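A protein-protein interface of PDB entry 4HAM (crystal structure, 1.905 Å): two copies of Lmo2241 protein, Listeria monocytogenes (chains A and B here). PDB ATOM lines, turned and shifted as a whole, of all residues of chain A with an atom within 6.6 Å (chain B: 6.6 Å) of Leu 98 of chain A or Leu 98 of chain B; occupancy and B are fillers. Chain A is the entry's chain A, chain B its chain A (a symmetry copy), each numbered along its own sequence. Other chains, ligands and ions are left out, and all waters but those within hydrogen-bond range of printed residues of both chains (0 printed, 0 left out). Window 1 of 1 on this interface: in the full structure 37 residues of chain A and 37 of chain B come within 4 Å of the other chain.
Printed residues of chain B within 4 Å of Leu 98 of chain A: Leu 98, Thr 101 and Leu 118.
Printed residues of chain B within 4 Å of Thr 101 of chain A: Thr 94 (3.7 Å) and Leu 98 (3.7 Å).
Of the printed residues of chain A, Lys 99 of chain B touches Tyr 122 (3.7 Å) and Ile 126 (3.8 Å).
Of the printed residues of chain A, Thr 101 of chain B touches Thr 94 (3.7 Å) and Leu 98 (3.7 Å).
Leu 98 of chain A touches Leu 98 of chain B.
Leu 98 of chain A touches Leu 118 of chain B (CD2 to CB, 3.9 Å).
Thr 101 of chain A touches Thr 94 of chain B (CG2 to O, 3.7 Å).
Ala 119 of chain B touches Ile 102 of chain A (CA to CD1, 3.6 Å).
Ile 102 of chain A touches Ile 126 of chain B (CG2 to CD1, 3.7 Å).
Ile 126 of chain B touches Leu 103 of chain A.
Ile 102 of chain B touches Ala 119 of chain A.
Tyr 122 of chain A touches Lys 99 of chain B.
CD1 of Ile 126 of chain A touches O of Lys 99 of chain B, 3.8 Å away.
Ile 126 of chain A touches Leu 103 of chain B.
Arg 95 of chain A touches Tyr 122 of chain B, and with the chains exchanged Tyr 122 of chain A touches Arg 95 of chain B.
Leu 98 of chain A touches Thr 101 of chain B, and with the chains exchanged Thr 101 of chain A touches Leu 98 of chain B.
Ile 102 of chain A touches Ala 119 of chain B, and with the chains exchanged Ala 119 of chain A touches Ile 102 of chain B.
Leu 103 of chain A touches Ile 126 of chain B, and with the chains exchanged Ile 126 of chain A touches Leu 103 of chain B.
Positions printed for both chains: 93, 94, 95, 96, 97, 98, 99, 100, 101, 102, 103, 105, 114, 115, 118, 119, 122 and 126.
Of the 21 pairs that touch across the chains among the printed residues, 21 have their exchanged pair printed and touching as well.
The backbone carbonyl oxygen of Lys 97 of chain A sits at hydrogen-bond distance from the side-chain hydroxyl of Thr 101 of chain A (2.6 Å).
The backbone carbonyl oxygen (O) of Lys 97 of chain B is in hydrogen-bond range of the side-chain hydroxyl (OG1) of Thr 101 of chain B (2.6 Å).
Of the 18 printed residues of chain A, 12 touch a printed residue of chain B.
Hydrophobic or aromatic side chains of chain A within 4 Å of the printed part of chain B: Leu 98, Ile 102, Leu 103, Leu 105, Leu 118, Ala 119, Tyr 122 and Ile 126.
Among the printed residues, 21 pairs touch across the chains.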
ATOM      1  N   GLU A  93      12.887  13.246 -11.269  1.00  0.00           N
ATOM      2  CA  GLU A  93      12.827  14.054 -10.054  1.00  0.00           C
ATOM      3  C   GLU A  93      13.922  15.114 -10.030  1.00  0.00           C
ATOM      4  O   GLU A  93      13.711  16.231  -9.558  1.00  0.00           O
ATOM      5  CB  GLU A  93      12.950  13.159  -8.824  1.00  0.00           C
ATOM      6  CG  GLU A  93      11.695  12.373  -8.532  1.00  0.00           C
ATOM      7  CD  GLU A  93      11.900  11.320  -7.461  1.00  0.00           C
ATOM      8  OE1 GLU A  93      13.058  11.119  -7.018  1.00  0.00           O
ATOM      9  OE2 GLU A  93      10.896  10.684  -7.070  1.00  0.00           O
ATOM     10  N   THR A  94      15.093  14.753 -10.540  1.00  0.00           N
ATOM     11  CA  THR A  94      16.238  15.652 -10.527  1.00  0.00           C
ATOM     12  C   THR A  94      16.062  16.751 -11.560  1.00  0.00           C
ATOM     13  O   THR A  94      16.408  17.905 -11.309  1.00  0.00           O
ATOM     14  CB  THR A  94      17.560  14.886 -10.751  1.00  0.00           C
ATOM     15  OG1 THR A  94      17.680  13.846  -9.771  1.00  0.00           O
ATOM     16  CG2 THR A  94      18.749  15.836 -10.600  1.00  0.00           C
ATOM     17  N   ARG A  95      15.487  16.410 -12.712  1.00  0.00           N
ATOM     18  CA  ARG A  95      15.144  17.424 -13.715  1.00  0.00           C
ATOM     19  C   ARG A  95      14.131  18.435 -13.184  1.00  0.00           C
ATOM     20  O   ARG A  95      14.214  19.629 -13.475  1.00  0.00           O
ATOM     21  CB  ARG A  95      14.635  16.770 -15.013  1.00  0.00           C
ATOM     22  CG  ARG A  95      15.743  16.122 -15.837  1.00  0.00           C
ATOM     23  CD  ARG A  95      15.267  15.777 -17.242  1.00  0.00           C
ATOM     24  NE  ARG A  95      14.231  14.759 -17.211  1.00  0.00           N
ATOM     25  CZ  ARG A  95      14.443  13.470 -17.449  1.00  0.00           C
ATOM     26  NH1 ARG A  95      13.432  12.619 -17.388  1.00  0.00           N
ATOM     27  NH2 ARG A  95      15.660  13.038 -17.747  1.00  0.00           N
ATOM     28  N   THR A  96      13.161  17.959 -12.416  1.00  0.00           N
ATOM     29  CA  THR A  96      12.204  18.866 -11.780  1.00  0.00           C
ATOM     30  C   THR A  96      12.930  19.813 -10.821  1.00  0.00           C
ATOM     31  O   THR A  96      12.655  21.013 -10.794  1.00  0.00           O
ATOM     32  CB  THR A  96      11.099  18.091 -11.043  1.00  0.00           C
ATOM     33  OG1 THR A  96      10.282  17.428 -12.009  1.00  0.00           O
ATOM     34  CG2 THR A  96      10.212  19.040 -10.225  1.00  0.00           C
ATOM     35  N   LYS A  97      13.885  19.281 -10.064  1.00  0.00           N
ATOM     36  CA  LYS A  97      14.658  20.114  -9.144  1.00  0.00           C
ATOM     37  C   LYS A  97      15.454  21.175  -9.892  1.00  0.00           C
ATOM     38  O   LYS A  97      15.607  22.290  -9.406  1.00  0.00           O
ATOM     39  CB  LYS A  97      15.595  19.274  -8.287  1.00  0.00           C
ATOM     40  CG  LYS A  97      14.884  18.414  -7.250  1.00  0.00           C
ATOM     41  CD  LYS A  97      15.873  17.515  -6.529  1.00  0.00           C
ATOM     42  CE  LYS A  97      15.175  16.379  -5.796  1.00  0.00           C
ATOM     43  NZ  LYS A  97      16.173  15.384  -5.303  1.00  0.00           N
ATOM     44  N   LEU A  98      15.968  20.820 -11.069  1.00  0.00           N
ATOM     45  CA  LEU A  98      16.676  21.781 -11.899  1.00  0.00           C
ATOM     46  C   LEU A  98      15.728  22.889 -12.338  1.00  0.00           C
ATOM     47  O   LEU A  98      16.061  24.081 -12.284  1.00  0.00           O
ATOM     48  CB  LEU A  98      17.271  21.098 -13.138  1.00  0.00           C
ATOM     49  CG  LEU A  98      18.087  22.066 -13.998  1.00  0.00           C
ATOM     50  CD1 LEU A  98      19.250  22.618 -13.180  1.00  0.00           C
ATOM     51  CD2 LEU A  98      18.600  21.412 -15.264  1.00  0.00           C
ATOM     52  N   LYS A  99      14.537  22.495 -12.767  1.00  0.00           N
ATOM     53  CA  LYS A  99      13.571  23.477 -13.237  1.00  0.00           C
ATOM     54  C   LYS A  99      13.200  24.469 -12.132  1.00  0.00           C
ATOM     55  O   LYS A  99      13.222  25.688 -12.350  1.00  0.00           O
ATOM     56  CB  LYS A  99      12.320  22.808 -13.817  1.00  0.00           C
ATOM     57  CG  LYS A  99      11.345  23.825 -14.352  1.00  0.00           C
ATOM     58  CD  LYS A  99      10.303  23.214 -15.259  1.00  0.00           C
ATOM     59  CE  LYS A  99       9.512  24.325 -15.921  1.00  0.00           C
ATOM     60  NZ  LYS A  99       8.380  23.795 -16.731  1.00  0.00           N
ATOM     61  N   GLU A 100      12.890  23.939 -10.953  1.00  0.00           N
ATOM     62  CA  GLU A 100      12.485  24.759  -9.823  1.00  0.00           C
ATOM     63  C   GLU A 100      13.609  25.709  -9.392  1.00  0.00           C
ATOM     64  O   GLU A 100      13.358  26.861  -9.036  1.00  0.00           O
ATOM     65  CB  GLU A 100      12.021  23.874  -8.664  1.00  0.00           C
ATOM     66  CG  GLU A 100      10.732  23.089  -8.958  1.00  0.00           C
ATOM     67  CD  GLU A 100       9.517  23.992  -9.175  1.00  0.00           C
ATOM     68  OE1 GLU A 100       9.506  25.132  -8.659  1.00  0.00           O
ATOM     69  OE2 GLU A 100       8.563  23.567  -9.865  1.00  0.00           O
ATOM     70  N   THR A 101      14.844  25.224  -9.460  1.00  0.00           N
ATOM     71  CA  THR A 101      16.007  26.008  -9.068  1.00  0.00           C
ATOM     72  C   THR A 101      16.225  27.153 -10.048  1.00  0.00           C
ATOM     73  O   THR A 101      16.511  28.286  -9.654  1.00  0.00           O
ATOM     74  CB  THR A 101      17.271  25.135  -9.010  1.00  0.00           C
ATOM     75  OG1 THR A 101      17.054  24.062  -8.086  1.00  0.00           O
ATOM     76  CG2 THR A 101      18.461  25.961  -8.553  1.00  0.00           C
ATOM     77  N   ILE A 102      16.082  26.850 -11.331  1.00  0.00           N
ATOM     78  CA  ILE A 102      16.162  27.884 -12.351  1.00  0.00           C
ATOM     79  C   ILE A 102      15.074  28.946 -12.163  1.00  0.00           C
ATOM     80  O   ILE A 102      15.352  30.144 -12.257  1.00  0.00           O
ATOM     81  CB  ILE A 102      16.118  27.275 -13.749  1.00  0.00           C
ATOM     82  CG1 ILE A 102      17.447  26.555 -14.024  1.00  0.00           C
ATOM     83  CG2 ILE A 102      15.821  28.347 -14.812  1.00  0.00           C
ATOM     84  CD1 ILE A 102      17.452  25.754 -15.292  1.00  0.00           C
ATOM     85  N   LEU A 103      13.846  28.516 -11.883  1.00  0.00           N
ATOM     86  CA  LEU A 103      12.782  29.474 -11.587  1.00  0.00           C
ATOM     87  C   LEU A 103      13.189  30.385 -10.427  1.00  0.00           C
ATOM     88  O   LEU A 103      12.994  31.606 -10.484  1.00  0.00           O
ATOM     89  CB  LEU A 103      11.476  28.758 -11.263  1.00  0.00           C
ATOM     90  CG  LEU A 103      10.354  29.631 -10.688  1.00  0.00           C
ATOM     91  CD1 LEU A 103       9.942  30.728 -11.671  1.00  0.00           C
ATOM     92  CD2 LEU A 103       9.174  28.775 -10.312  1.00  0.00           C
ATOM     93  N   LEU A 105      16.245  31.201  -9.254  1.00  0.00           N
ATOM     94  CA  LEU A 105      17.299  32.109  -9.675  1.00  0.00           C
ATOM     95  C   LEU A 105      16.747  33.233 -10.569  1.00  0.00           C
ATOM     96  O   LEU A 105      17.059  34.400 -10.362  1.00  0.00           O
ATOM     97  CB  LEU A 105      18.393  31.343 -10.426  1.00  0.00           C
ATOM     98  CG  LEU A 105      19.230  30.357  -9.608  1.00  0.00           C
ATOM     99  CD1 LEU A 105      20.025  29.445 -10.528  1.00  0.00           C
ATOM    100  CD2 LEU A 105      20.157  31.088  -8.636  1.00  0.00           C
ATOM    101  N   GLU A 114      24.103  34.122 -16.792  1.00  0.00           N
ATOM    102  CA  GLU A 114      24.742  33.910 -15.497  1.00  0.00           C
ATOM    103  C   GLU A 114      24.533  32.475 -15.006  1.00  0.00           C
ATOM    104  O   GLU A 114      25.414  31.886 -14.384  1.00  0.00           O
ATOM    105  CB  GLU A 114      24.213  34.921 -14.473  1.00  0.00           C
ATOM    106  CG  GLU A 114      24.582  36.362 -14.789  1.00  0.00           C
ATOM    107  CD  GLU A 114      23.894  37.381 -13.887  1.00  0.00           C
ATOM    108  OE1 GLU A 114      22.653  37.320 -13.735  1.00  0.00           O
ATOM    109  OE2 GLU A 114      24.600  38.254 -13.339  1.00  0.00           O
ATOM    110  N   ILE A 115      23.363  31.917 -15.293  1.00  0.00           N
ATOM    111  CA  ILE A 115      23.056  30.537 -14.936  1.00  0.00           C
ATOM    112  C   ILE A 115      23.939  29.525 -15.682  1.00  0.00           C
ATOM    113  O   ILE A 115      24.441  28.581 -15.073  1.00  0.00           O
ATOM    114  CB  ILE A 115      21.555  30.210 -15.145  1.00  0.00           C
ATOM    115  CG1 ILE A 115      20.709  30.989 -14.140  1.00  0.00           C
ATOM    116  CG2 ILE A 115      21.295  28.720 -14.980  1.00  0.00           C
ATOM    117  CD1 ILE A 115      19.213  30.918 -14.419  1.00  0.00           C
ATOM    118  N   LEU A 118      27.378  29.711 -14.011  1.00  0.00           N
ATOM    119  CA  LEU A 118      27.334  28.959 -12.762  1.00  0.00           C
ATOM    120  C   LEU A 118      27.360  27.458 -13.018  1.00  0.00           C
ATOM    121  O   LEU A 118      28.058  26.717 -12.321  1.00  0.00           O
ATOM    122  CB  LEU A 118      26.081  29.300 -11.956  1.00  0.00           C
ATOM    123  CG  LEU A 118      26.018  30.677 -11.293  1.00  0.00           C
ATOM    124  CD1 LEU A 118      24.662  30.873 -10.608  1.00  0.00           C
ATOM    125  CD2 LEU A 118      27.166  30.871 -10.306  1.00  0.00           C
ATOM    126  N   ALA A 119      26.594  26.999 -14.006  1.00  0.00           N
ATOM    127  CA  ALA A 119      26.534  25.564 -14.271  1.00  0.00           C
ATOM    128  C   ALA A 119      27.900  25.033 -14.685  1.00  0.00           C
ATOM    129  O   ALA A 119      28.336  23.969 -14.229  1.00  0.00           O
ATOM    130  CB  ALA A 119      25.484  25.248 -15.324  1.00  0.00           C
ATOM    131  N   TYR A 122      30.181  25.005 -11.476  1.00  0.00           N
ATOM    132  CA  TYR A 122      29.838  23.911 -10.563  1.00  0.00           C
ATOM    133  C   TYR A 122      30.190  22.554 -11.160  1.00  0.00           C
ATOM    134  O   TYR A 122      30.733  21.674 -10.479  1.00  0.00           O
ATOM    135  CB  TYR A 122      28.354  23.959 -10.200  1.00  0.00           C
ATOM    136  CG  TYR A 122      27.995  25.171  -9.379  1.00  0.00           C
ATOM    137  CD1 TYR A 122      28.963  25.831  -8.632  1.00  0.00           C
ATOM    138  CD2 TYR A 122      26.704  25.668  -9.362  1.00  0.00           C
ATOM    139  CE1 TYR A 122      28.649  26.944  -7.879  1.00  0.00           C
ATOM    140  CE2 TYR A 122      26.379  26.787  -8.602  1.00  0.00           C
ATOM    141  CZ  TYR A 122      27.354  27.421  -7.867  1.00  0.00           C
ATOM    142  OH  TYR A 122      27.047  28.537  -7.112  1.00  0.00           O
ATOM    143  N   ILE A 126      32.796  19.911  -9.547  1.00  0.00           N
ATOM    144  CA  ILE A 126      32.380  18.543  -9.276  1.00  0.00           C
ATOM    145  C   ILE A 126      33.328  17.538  -9.926  1.00  0.00           C
ATOM    146  O   ILE A 126      33.793  16.605  -9.272  1.00  0.00           O
ATOM    147  CB  ILE A 126      30.923  18.340  -9.738  1.00  0.00           C
ATOM    148  CG1 ILE A 126      29.989  19.028  -8.749  1.00  0.00           C
ATOM    149  CG2 ILE A 126      30.580  16.853  -9.882  1.00  0.00           C
ATOM    150  CD1 ILE A 126      28.619  19.372  -9.316  1.00  0.00           C
ATOM    151  N   GLU B  93      21.582  30.290  -0.935  1.00  0.00           N
ATOM    152  CA  GLU B  93      20.914  29.005  -0.751  1.00  0.00           C
ATOM    153  C   GLU B  93      20.499  28.391  -2.083  1.00  0.00           C
ATOM    154  O   GLU B  93      20.559  27.175  -2.264  1.00  0.00           O
ATOM    155  CB  GLU B  93      19.687  29.176   0.142  1.00  0.00           C
ATOM    156  CG  GLU B  93      20.032  29.366   1.599  1.00  0.00           C
ATOM    157  CD  GLU B  93      18.835  29.767   2.437  1.00  0.00           C
ATOM    158  OE1 GLU B  93      17.745  30.013   1.864  1.00  0.00           O
ATOM    159  OE2 GLU B  93      18.992  29.848   3.675  1.00  0.00           O
ATOM    160  N   THR B  94      20.074  29.241  -3.008  1.00  0.00           N
ATOM    161  CA  THR B  94      19.596  28.781  -4.303  1.00  0.00           C
ATOM    162  C   THR B  94      20.759  28.328  -5.169  1.00  0.00           C
ATOM    163  O   THR B  94      20.655  27.333  -5.885  1.00  0.00           O
ATOM    164  CB  THR B  94      18.761  29.866  -5.017  1.00  0.00           C
ATOM    165  OG1 THR B  94      17.687  30.280  -4.162  1.00  0.00           O
ATOM    166  CG2 THR B  94      18.165  29.306  -6.309  1.00  0.00           C
ATOM    167  N   ARG B  95      21.886  29.032  -5.080  1.00  0.00           N
ATOM    168  CA  ARG B  95      23.107  28.595  -5.765  1.00  0.00           C
ATOM    169  C   ARG B  95      23.585  27.232  -5.268  1.00  0.00           C
ATOM    170  O   ARG B  95      24.058  26.404  -6.046  1.00  0.00           O
ATOM    171  CB  ARG B  95      24.224  29.647  -5.636  1.00  0.00           C
ATOM    172  CG  ARG B  95      24.000  30.875  -6.512  1.00  0.00           C
ATOM    173  CD  ARG B  95      25.256  31.732  -6.607  1.00  0.00           C
ATOM    174  NE  ARG B  95      25.604  32.298  -5.315  1.00  0.00           N
ATOM    175  CZ  ARG B  95      25.324  33.542  -4.946  1.00  0.00           C
ATOM    176  NH1 ARG B  95      25.676  33.962  -3.742  1.00  0.00           N
ATOM    177  NH2 ARG B  95      24.693  34.360  -5.778  1.00  0.00           N
ATOM    178  N   THR B  96      23.480  27.003  -3.966  1.00  0.00           N
ATOM    179  CA  THR B  96      23.819  25.690  -3.414  1.00  0.00           C
ATOM    180  C   THR B  96      22.899  24.616  -4.000  1.00  0.00           C
ATOM    181  O   THR B  96      23.353  23.534  -4.372  1.00  0.00           O
ATOM    182  CB  THR B  96      23.742  25.690  -1.878  1.00  0.00           C
ATOM    183  OG1 THR B  96      24.795  26.508  -1.366  1.00  0.00           O
ATOM    184  CG2 THR B  96      23.912  24.271  -1.318  1.00  0.00           C
ATOM    185  N   LYS B  97      21.612  24.931  -4.120  1.00  0.00           N
ATOM    186  CA  LYS B  97      20.664  23.982  -4.702  1.00  0.00           C
ATOM    187  C   LYS B  97      21.010  23.671  -6.152  1.00  0.00           C
ATOM    188  O   LYS B  97      20.838  22.543  -6.600  1.00  0.00           O
ATOM    189  CB  LYS B  97      19.235  24.499  -4.612  1.00  0.00           C
ATOM    190  CG  LYS B  97      18.671  24.523  -3.197  1.00  0.00           C
ATOM    191  CD  LYS B  97      17.296  25.170  -3.178  1.00  0.00           C
ATOM    192  CE  LYS B  97      16.883  25.576  -1.772  1.00  0.00           C
ATOM    193  NZ  LYS B  97      15.650  26.417  -1.813  1.00  0.00           N
ATOM    194  N   LEU B  98      21.488  24.677  -6.883  1.00  0.00           N
ATOM    195  CA  LEU B  98      21.925  24.467  -8.254  1.00  0.00           C
ATOM    196  C   LEU B  98      23.116  23.518  -8.283  1.00  0.00           C
ATOM    197  O   LEU B  98      23.177  22.585  -9.095  1.00  0.00           O
ATOM    198  CB  LEU B  98      22.316  25.797  -8.912  1.00  0.00           C
ATOM    199  CG  LEU B  98      22.710  25.623 -10.381  1.00  0.00           C
ATOM    200  CD1 LEU B  98      21.529  25.059 -11.163  1.00  0.00           C
ATOM    201  CD2 LEU B  98      23.180  26.921 -11.004  1.00  0.00           C
ATOM    202  N   LYS B  99      24.063  23.753  -7.386  1.00  0.00           N
ATOM    203  CA  LYS B  99      25.257  22.919  -7.352  1.00  0.00           C
ATOM    204  C   LYS B  99      24.908  21.455  -7.073  1.00  0.00           C
ATOM    205  O   LYS B  99      25.370  20.554  -7.786  1.00  0.00           O
ATOM    206  CB  LYS B  99      26.284  23.441  -6.341  1.00  0.00           C
ATOM    207  CG  LYS B  99      27.540  22.609  -6.348  1.00  0.00           C
ATOM    208  CD  LYS B  99      28.700  23.297  -5.667  1.00  0.00           C
ATOM    209  CE  LYS B  99      29.963  22.496  -5.913  1.00  0.00           C
ATOM    210  NZ  LYS B  99      31.125  23.046  -5.161  1.00  0.00           N
ATOM    211  N   GLU B 100      24.078  21.237  -6.058  1.00  0.00           N
ATOM    212  CA  GLU B 100      23.687  19.895  -5.658  1.00  0.00           C
ATOM    213  C   GLU B 100      22.921  19.180  -6.778  1.00  0.00           C
ATOM    214  O   GLU B 100      23.102  17.982  -6.999  1.00  0.00           O
ATOM    215  CB  GLU B 100      22.875  19.943  -4.362  1.00  0.00           C
ATOM    216  CG  GLU B 100      23.681  20.411  -3.140  1.00  0.00           C
ATOM    217  CD  GLU B 100      24.816  19.456  -2.768  1.00  0.00           C
ATOM    218  OE1 GLU B 100      24.727  18.250  -3.093  1.00  0.00           O
ATOM    219  OE2 GLU B 100      25.806  19.905  -2.150  1.00  0.00           O
ATOM    220  N   THR B 101      22.094  19.933  -7.495  1.00  0.00           N
ATOM    221  CA  THR B 101      21.291  19.385  -8.580  1.00  0.00           C
ATOM    222  C   THR B 101      22.186  18.971  -9.740  1.00  0.00           C
ATOM    223  O   THR B 101      22.006  17.906 -10.338  1.00  0.00           O
ATOM    224  CB  THR B 101      20.253  20.407  -9.073  1.00  0.00           C
ATOM    225  OG1 THR B 101      19.418  20.789  -7.973  1.00  0.00           O
ATOM    226  CG2 THR B 101      19.395  19.799 -10.169  1.00  0.00           C
ATOM    227  N   ILE B 102      23.158  19.818 -10.052  1.00  0.00           N
ATOM    228  CA  ILE B 102      24.139  19.479 -11.072  1.00  0.00           C
ATOM    229  C   ILE B 102      24.933  18.224 -10.694  1.00  0.00           C
ATOM    230  O   ILE B 102      25.141  17.345 -11.534  1.00  0.00           O
ATOM    231  CB  ILE B 102      25.058  20.662 -11.357  1.00  0.00           C
ATOM    232  CG1 ILE B 102      24.269  21.737 -12.121  1.00  0.00           C
ATOM    233  CG2 ILE B 102      26.310  20.217 -12.132  1.00  0.00           C
ATOM    234  CD1 ILE B 102      25.012  23.028 -12.292  1.00  0.00           C
ATOM    235  N   LEU B 103      25.363  18.130  -9.439  1.00  0.00           N
ATOM    236  CA  LEU B 103      26.034  16.915  -8.981  1.00  0.00           C
ATOM    237  C   LEU B 103      25.150  15.691  -9.222  1.00  0.00           C
ATOM    238  O   LEU B 103      25.623  14.653  -9.700  1.00  0.00           O
ATOM    239  CB  LEU B 103      26.406  17.018  -7.506  1.00  0.00           C
ATOM    240  CG  LEU B 103      26.882  15.722  -6.840  1.00  0.00           C
ATOM    241  CD1 LEU B 103      28.151  15.187  -7.506  1.00  0.00           C
ATOM    242  CD2 LEU B 103      27.101  15.947  -5.368  1.00  0.00           C
ATOM    243  N   LEU B 105      22.614  15.216 -11.395  1.00  0.00           N
ATOM    244  CA  LEU B 105      22.518  14.937 -12.819  1.00  0.00           C
ATOM    245  C   LEU B 105      23.814  14.301 -13.353  1.00  0.00           C
ATOM    246  O   LEU B 105      23.767  13.307 -14.070  1.00  0.00           O
ATOM    247  CB  LEU B 105      22.219  16.224 -13.594  1.00  0.00           C
ATOM    248  CG  LEU B 105      20.842  16.856 -13.375  1.00  0.00           C
ATOM    249  CD1 LEU B 105      20.814  18.271 -13.929  1.00  0.00           C
ATOM    250  CD2 LEU B 105      19.735  16.007 -14.000  1.00  0.00           C
ATOM    251  N   GLU B 114      24.219  18.503 -22.059  1.00  0.00           N
ATOM    252  CA  GLU B 114      22.804  18.207 -21.861  1.00  0.00           C
ATOM    253  C   GLU B 114      22.195  19.106 -20.781  1.00  0.00           C
ATOM    254  O   GLU B 114      21.041  19.515 -20.877  1.00  0.00           O
ATOM    255  CB  GLU B 114      22.617  16.726 -21.508  1.00  0.00           C
ATOM    256  CG  GLU B 114      22.997  15.777 -22.635  1.00  0.00           C
ATOM    257  CD  GLU B 114      23.002  14.309 -22.221  1.00  0.00           C
ATOM    258  OE1 GLU B 114      23.629  13.967 -21.193  1.00  0.00           O
ATOM    259  OE2 GLU B 114      22.383  13.493 -22.937  1.00  0.00           O
ATOM    260  N   ILE B 115      22.982  19.412 -19.757  1.00  0.00           N
ATOM    261  CA  ILE B 115      22.549  20.306 -18.690  1.00  0.00           C
ATOM    262  C   ILE B 115      22.311  21.741 -19.183  1.00  0.00           C
ATOM    263  O   ILE B 115      21.306  22.355 -18.826  1.00  0.00           O
ATOM    264  CB  ILE B 115      23.538  20.297 -17.495  1.00  0.00           C
ATOM    265  CG1 ILE B 115      23.499  18.939 -16.800  1.00  0.00           C
ATOM    266  CG2 ILE B 115      23.192  21.389 -16.495  1.00  0.00           C
ATOM    267  CD1 ILE B 115      24.604  18.752 -15.767  1.00  0.00           C
ATOM    268  N   LEU B 118      19.007  21.644 -21.114  1.00  0.00           N
ATOM    269  CA  LEU B 118      17.905  21.643 -20.159  1.00  0.00           C
ATOM    270  C   LEU B 118      17.697  23.026 -19.554  1.00  0.00           C
ATOM    271  O   LEU B 118      16.559  23.478 -19.404  1.00  0.00           O
ATOM    272  CB  LEU B 118      18.152  20.643 -19.030  1.00  0.00           C
ATOM    273  CG  LEU B 118      18.046  19.155 -19.368  1.00  0.00           C
ATOM    274  CD1 LEU B 118      18.409  18.308 -18.144  1.00  0.00           C
ATOM    275  CD2 LEU B 118      16.655  18.802 -19.888  1.00  0.00           C
ATOM    276  N   ALA B 119      18.788  23.698 -19.191  1.00  0.00           N
ATOM    277  CA  ALA B 119      18.656  25.007 -18.556  1.00  0.00           C
ATOM    278  C   ALA B 119      17.997  26.002 -19.503  1.00  0.00           C
ATOM    279  O   ALA B 119      17.117  26.774 -19.104  1.00  0.00           O
ATOM    280  CB  ALA B 119      20.006  25.520 -18.080  1.00  0.00           C
ATOM    281  N   TYR B 122      14.192  25.030 -19.780  1.00  0.00           N
ATOM    282  CA  TYR B 122      13.437  25.404 -18.580  1.00  0.00           C
ATOM    283  C   TYR B 122      13.323  26.917 -18.441  1.00  0.00           C
ATOM    284  O   TYR B 122      12.256  27.452 -18.114  1.00  0.00           O
ATOM    285  CB  TYR B 122      14.083  24.805 -17.331  1.00  0.00           C
ATOM    286  CG  TYR B 122      13.996  23.301 -17.295  1.00  0.00           C
ATOM    287  CD1 TYR B 122      13.014  22.631 -18.015  1.00  0.00           C
ATOM    288  CD2 TYR B 122      14.898  22.549 -16.564  1.00  0.00           C
ATOM    289  CE1 TYR B 122      12.925  21.255 -17.995  1.00  0.00           C
ATOM    290  CE2 TYR B 122      14.813  21.161 -16.534  1.00  0.00           C
ATOM    291  CZ  TYR B 122      13.829  20.521 -17.252  1.00  0.00           C
ATOM    292  OH  TYR B 122      13.735  19.142 -17.238  1.00  0.00           O
ATOM    293  N   ILE B 126       9.847  28.989 -18.382  1.00  0.00           N
ATOM    294  CA  ILE B 126       9.548  29.888 -17.277  1.00  0.00           C
ATOM    295  C   ILE B 126       9.200  31.286 -17.780  1.00  0.00           C
ATOM    296  O   ILE B 126       8.187  31.860 -17.381  1.00  0.00           O
ATOM    297  CB  ILE B 126      10.732  29.912 -16.288  1.00  0.00           C
ATOM    298  CG1 ILE B 126      10.735  28.614 -15.489  1.00  0.00           C
ATOM    299  CG2 ILE B 126      10.668  31.132 -15.363  1.00  0.00           C
ATOM    300  CD1 ILE B 126      12.085  28.255 -14.881  1.00  0.00           C
